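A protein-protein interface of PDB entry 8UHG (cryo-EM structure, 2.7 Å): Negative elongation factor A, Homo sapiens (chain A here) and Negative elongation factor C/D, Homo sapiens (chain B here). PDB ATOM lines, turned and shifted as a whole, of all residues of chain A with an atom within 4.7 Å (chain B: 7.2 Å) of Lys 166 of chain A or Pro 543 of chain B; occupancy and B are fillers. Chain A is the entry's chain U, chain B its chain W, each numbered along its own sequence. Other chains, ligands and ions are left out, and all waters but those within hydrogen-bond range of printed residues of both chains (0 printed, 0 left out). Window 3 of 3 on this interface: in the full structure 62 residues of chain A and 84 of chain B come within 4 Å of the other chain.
The backbone carbonyl oxygen (O) of Ile 541 of chain B sits at hydrogen-bond distance from the side-chain hydroxyl (OH) of Tyr 545 of chain B (2.8 Å).
The backbone carbonyl oxygen (O) of Asp 539 of chain B sits close to the guanidinium group (NH1) of Arg 167 of chain A.
NH1 of Arg 167 of chain A lies within hydrogen-bond range of O of Val 540 of chain B (2.9 Å).
Printed residues of chain B within 4 Å of Gln 164 of chain A: Ala 542 (3.4 Å).
Lys 166 of chain A touches just these residues of chain B: Ile 541, Ala 542 and Pro 543.
Of the printed residues of chain B, Arg 167 of chain A touches Asp 539 (3.0 Å) and Val 540 (2.9 Å).
Of the printed residues of chain A, Ile 541 of chain B touches Lys 166 (3.8 Å).
Of the printed residues of chain A, Ala 542 of chain B touches Phe 163, Gln 164 and Lys 166.
Of chain A, only Lys 166 comes within 4 Å of Pro 543 of chain B.
Of the printed residues of chain A, Pro 544 of chain B touches Phe 163.
The nearest residue of chain B that does not touch Lys 166 of chain A is Val 540 of chain B (4.7 Å).
The nearest printed residue of chain A that does not touch Ile 541 of chain B is Arg 167 of chain A (4.3 Å).
Hydrophobic or aromatic side chains of chain B within 4 Å of the printed part of chain A: Ala 542 and Pro 543.
Hydrophobic or aromatic side chains of chain A within 4 Å of the printed part of chain B: Phe 163.
Among the printed residues, 8 pairs touch across the chains.
Among the printed residues, no Asp or Glu carboxylate lies within 4 Å of a Lys or Arg side-chain nitrogen of the other chain.
Ala 542 of chain B touches Phe 163 of chain A.
Phe 163 of chain A touches Pro 544 of chain B.
Ala 542 of chain B touches Gln 164 of chain A.
NZ of Lys 166 of chain A touches O of Ile 541 of chain B, 3.8 Å away.
NZ of Lys 166 of chain A touches CA of Ala 542 of chain B, at 3.6 Å.
Lys 166 of chain A touches Pro 543 of chain B.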
ATOM      1  N   PHE A 163      -6.502  10.355  14.389  1.00  0.00           N
ATOM      2  CA  PHE A 163      -6.807  11.488  15.250  1.00  0.00           C
ATOM      3  C   PHE A 163      -7.697  12.452  14.483  1.00  0.00           C
ATOM      4  O   PHE A 163      -7.603  12.557  13.257  1.00  0.00           O
ATOM      5  CB  PHE A 163      -5.529  12.200  15.711  1.00  0.00           C
ATOM      6  CG  PHE A 163      -4.542  12.453  14.603  1.00  0.00           C
ATOM      7  CD1 PHE A 163      -4.653  13.571  13.790  1.00  0.00           C
ATOM      8  CD2 PHE A 163      -3.499  11.571  14.378  1.00  0.00           C
ATOM      9  CE1 PHE A 163      -3.747  13.799  12.773  1.00  0.00           C
ATOM     10  CE2 PHE A 163      -2.591  11.795  13.362  1.00  0.00           C
ATOM     11  CZ  PHE A 163      -2.714  12.909  12.559  1.00  0.00           C
ATOM     12  N   GLN A 164      -8.555  13.155  15.215  1.00  0.00           N
ATOM     13  CA  GLN A 164      -9.361  14.205  14.616  1.00  0.00           C
ATOM     14  C   GLN A 164      -8.506  15.450  14.417  1.00  0.00           C
ATOM     15  O   GLN A 164      -7.731  15.837  15.297  1.00  0.00           O
ATOM     16  CB  GLN A 164     -10.576  14.522  15.494  1.00  0.00           C
ATOM     17  CG  GLN A 164     -11.717  15.249  14.773  1.00  0.00           C
ATOM     18  CD  GLN A 164     -11.484  16.746  14.639  1.00  0.00           C
ATOM     19  OE1 GLN A 164     -11.109  17.414  15.602  1.00  0.00           O
ATOM     20  NE2 GLN A 164     -11.699  17.275  13.440  1.00  0.00           N
ATOM     21  N   LEU A 165      -8.653  16.076  13.254  1.00  0.00           N
ATOM     22  CA  LEU A 165      -7.870  17.258  12.916  1.00  0.00           C
ATOM     23  C   LEU A 165      -8.405  18.458  13.688  1.00  0.00           C
ATOM     24  O   LEU A 165      -9.558  18.857  13.498  1.00  0.00           O
ATOM     25  CB  LEU A 165      -7.931  17.521  11.412  1.00  0.00           C
ATOM     26  CG  LEU A 165      -7.351  16.440  10.495  1.00  0.00           C
ATOM     27  CD1 LEU A 165      -7.835  16.637   9.065  1.00  0.00           C
ATOM     28  CD2 LEU A 165      -5.830  16.445  10.545  1.00  0.00           C
ATOM     29  N   LYS A 166      -7.571  19.035  14.559  1.00  0.00           N
ATOM     30  CA  LYS A 166      -7.984  20.240  15.271  1.00  0.00           C
ATOM     31  C   LYS A 166      -7.991  21.479  14.381  1.00  0.00           C
ATOM     32  O   LYS A 166      -8.539  22.508  14.793  1.00  0.00           O
ATOM     33  CB  LYS A 166      -7.086  20.479  16.497  1.00  0.00           C
ATOM     34  CG  LYS A 166      -5.606  20.856  16.230  1.00  0.00           C
ATOM     35  CD  LYS A 166      -4.958  21.490  17.460  1.00  0.00           C
ATOM     36  CE  LYS A 166      -4.680  20.485  18.570  1.00  0.00           C
ATOM     37  NZ  LYS A 166      -3.237  20.121  18.632  1.00  0.00           N
ATOM     38  N   ARG A 167      -7.404  21.408  13.189  1.00  0.00           N
ATOM     39  CA  ARG A 167      -7.309  22.538  12.278  1.00  0.00           C
ATOM     40  C   ARG A 167      -7.403  21.995  10.857  1.00  0.00           C
ATOM     41  O   ARG A 167      -7.648  20.803  10.646  1.00  0.00           O
ATOM     42  CB  ARG A 167      -6.007  23.316  12.523  1.00  0.00           C
ATOM     43  CG  ARG A 167      -4.739  22.475  12.369  1.00  0.00           C
ATOM     44  CD  ARG A 167      -3.484  23.315  12.493  1.00  0.00           C
ATOM     45  NE  ARG A 167      -3.293  23.864  13.831  1.00  0.00           N
ATOM     46  CZ  ARG A 167      -2.915  23.171  14.900  1.00  0.00           C
ATOM     47  NH1 ARG A 167      -2.737  21.858  14.858  1.00  0.00           N
ATOM     48  NH2 ARG A 167      -2.703  23.814  16.045  1.00  0.00           N
ATOM     49  N   LEU B 538       4.422  19.099  14.830  1.00  0.00           N
ATOM     50  CA  LEU B 538       3.828  19.385  16.131  1.00  0.00           C
ATOM     51  C   LEU B 538       3.026  20.680  16.130  1.00  0.00           C
ATOM     52  O   LEU B 538       2.213  20.888  17.038  1.00  0.00           O
ATOM     53  CB  LEU B 538       4.921  19.434  17.202  1.00  0.00           C
ATOM     54  CG  LEU B 538       5.862  18.223  17.255  1.00  0.00           C
ATOM     55  CD1 LEU B 538       6.864  18.375  18.381  1.00  0.00           C
ATOM     56  CD2 LEU B 538       5.106  16.918  17.389  1.00  0.00           C
ATOM     57  N   ASP B 539       3.224  21.553  15.136  1.00  0.00           N
ATOM     58  CA  ASP B 539       2.327  22.678  14.945  1.00  0.00           C
ATOM     59  C   ASP B 539       1.004  22.285  14.292  1.00  0.00           C
ATOM     60  O   ASP B 539       0.027  23.023  14.465  1.00  0.00           O
ATOM     61  CB  ASP B 539       3.023  23.755  14.107  1.00  0.00           C
ATOM     62  CG  ASP B 539       2.201  25.023  13.986  1.00  0.00           C
ATOM     63  OD1 ASP B 539       1.824  25.589  15.034  1.00  0.00           O
ATOM     64  OD2 ASP B 539       1.933  25.455  12.845  1.00  0.00           O
ATOM     65  N   VAL B 540       0.937  21.147  13.572  1.00  0.00           N
ATOM     66  CA  VAL B 540      -0.293  20.762  12.867  1.00  0.00           C
ATOM     67  C   VAL B 540      -0.955  19.490  13.405  1.00  0.00           C
ATOM     68  O   VAL B 540      -2.188  19.389  13.375  1.00  0.00           O
ATOM     69  CB  VAL B 540      -0.062  20.628  11.344  1.00  0.00           C
ATOM     70  CG1 VAL B 540       0.461  21.945  10.751  1.00  0.00           C
ATOM     71  CG2 VAL B 540       0.834  19.443  10.989  1.00  0.00           C
ATOM     72  N   ILE B 541      -0.184  18.513  13.909  1.00  0.00           N
ATOM     73  CA  ILE B 541      -0.797  17.245  14.315  1.00  0.00           C
ATOM     74  C   ILE B 541      -1.413  17.393  15.701  1.00  0.00           C
ATOM     75  O   ILE B 541      -0.824  18.000  16.604  1.00  0.00           O
ATOM     76  CB  ILE B 541       0.201  16.063  14.246  1.00  0.00           C
ATOM     77  CG1 ILE B 541       1.371  16.148  15.255  1.00  0.00           C
ATOM     78  CG2 ILE B 541       0.734  15.924  12.819  1.00  0.00           C
ATOM     79  CD1 ILE B 541       2.137  14.825  15.397  1.00  0.00           C
ATOM     80  N   ALA B 542      -2.616  16.836  15.866  1.00  0.00           N
ATOM     81  CA  ALA B 542      -3.411  16.880  17.087  1.00  0.00           C
ATOM     82  C   ALA B 542      -3.259  15.581  17.875  1.00  0.00           C
ATOM     83  O   ALA B 542      -3.268  14.500  17.275  1.00  0.00           O
ATOM     84  CB  ALA B 542      -4.888  17.085  16.755  1.00  0.00           C
ATOM     85  N   PRO B 543      -3.105  15.567  19.202  1.00  0.00           N
ATOM     86  CA  PRO B 543      -3.075  14.279  19.917  1.00  0.00           C
ATOM     87  C   PRO B 543      -4.433  13.600  19.867  1.00  0.00           C
ATOM     88  O   PRO B 543      -5.447  14.260  19.593  1.00  0.00           O
ATOM     89  CB  PRO B 543      -2.700  14.671  21.355  1.00  0.00           C
ATOM     90  CG  PRO B 543      -2.104  16.018  21.256  1.00  0.00           C
ATOM     91  CD  PRO B 543      -2.783  16.685  20.108  1.00  0.00           C
ATOM     92  N   PRO B 544      -4.508  12.281  20.124  1.00  0.00           N
ATOM     93  CA  PRO B 544      -3.436  11.340  20.492  1.00  0.00           C
ATOM     94  C   PRO B 544      -2.549  10.951  19.316  1.00  0.00           C
ATOM     95  O   PRO B 544      -2.969  11.013  18.163  1.00  0.00           O
ATOM     96  CB  PRO B 544      -4.215  10.133  21.027  1.00  0.00           C
ATOM     97  CG  PRO B 544      -5.477  10.140  20.225  1.00  0.00           C
ATOM     98  CD  PRO B 544      -5.814  11.600  20.039  1.00  0.00           C
ATOM     99  N   TYR B 545      -1.315  10.543  19.610  1.00  0.00           N
ATOM    100  CA  TYR B 545      -0.330  10.134  18.615  1.00  0.00           C
ATOM    101  C   TYR B 545      -0.090   8.640  18.782  1.00  0.00           C
ATOM    102  O   TYR B 545       0.475   8.206  19.792  1.00  0.00           O
ATOM    103  CB  TYR B 545       0.963  10.929  18.780  1.00  0.00           C
ATOM    104  CG  TYR B 545       0.755  12.428  18.780  1.00  0.00           C
ATOM    105  CD1 TYR B 545       0.007  13.044  17.789  1.00  0.00           C
ATOM    106  CD2 TYR B 545       1.293  13.224  19.780  1.00  0.00           C
ATOM    107  CE1 TYR B 545      -0.190  14.407  17.790  1.00  0.00           C
ATOM    108  CE2 TYR B 545       1.100  14.591  19.787  1.00  0.00           C
ATOM    109  CZ  TYR B 545       0.362  15.177  18.786  1.00  0.00           C
ATOM    110  OH  TYR B 545       0.165  16.538  18.786  1.00  0.00           O
ATOM    111  N   GLU B 577       6.373  18.945  25.124  1.00  0.00           N
ATOM    112  CA  GLU B 577       5.037  18.391  25.316  1.00  0.00           C
ATOM    113  C   GLU B 577       4.871  17.088  24.548  1.00  0.00           C
ATOM    114  O   GLU B 577       4.327  16.112  25.081  1.00  0.00           O
ATOM    115  CB  GLU B 577       3.983  19.411  24.871  1.00  0.00           C
ATOM    116  CG  GLU B 577       2.526  18.952  24.998  1.00  0.00           C
ATOM    117  CD  GLU B 577       1.543  20.025  24.578  1.00  0.00           C
ATOM    118  OE1 GLU B 577       1.859  20.786  23.639  1.00  0.00           O
ATOM    119  OE2 GLU B 577       0.455  20.107  25.186  1.00  0.00           O
ATOM    120  N   PHE B 578       5.334  17.055  23.297  1.00  0.00           N
ATOM    121  CA  PHE B 578       5.197  15.853  22.482  1.00  0.00           C
ATOM    122  C   PHE B 578       5.959  14.688  23.093  1.00  0.00           C
ATOM    123  O   PHE B 578       5.427  13.577  23.208  1.00  0.00           O
ATOM    124  CB  PHE B 578       5.694  16.124  21.061  1.00  0.00           C
ATOM    125  CG  PHE B 578       5.704  14.903  20.178  1.00  0.00           C
ATOM    126  CD1 PHE B 578       4.547  14.484  19.547  1.00  0.00           C
ATOM    127  CD2 PHE B 578       6.869  14.176  19.981  1.00  0.00           C
ATOM    128  CE1 PHE B 578       4.550  13.377  18.725  1.00  0.00           C
ATOM    129  CE2 PHE B 578       6.871  13.057  19.181  1.00  0.00           C
ATOM    130  CZ  PHE B 578       5.712  12.657  18.549  1.00  0.00           C
ATOM    131  N   HIS B 581       4.274  13.527  26.395  1.00  0.00           N
ATOM    132  CA  HIS B 581       3.022  12.816  26.157  1.00  0.00           C
ATOM    133  C   HIS B 581       3.271  11.445  25.545  1.00  0.00           C
ATOM    134  O   HIS B 581       2.624  10.461  25.926  1.00  0.00           O
ATOM    135  CB  HIS B 581       2.113  13.645  25.248  1.00  0.00           C
ATOM    136  CG  HIS B 581       0.858  12.936  24.837  1.00  0.00           C
ATOM    137  ND1 HIS B 581      -0.280  12.926  25.615  1.00  0.00           N
ATOM    138  CD2 HIS B 581       0.564  12.212  23.732  1.00  0.00           C
ATOM    139  CE1 HIS B 581      -1.221  12.228  25.005  1.00  0.00           C
ATOM    140  NE2 HIS B 581      -0.734  11.782  23.861  1.00  0.00           N
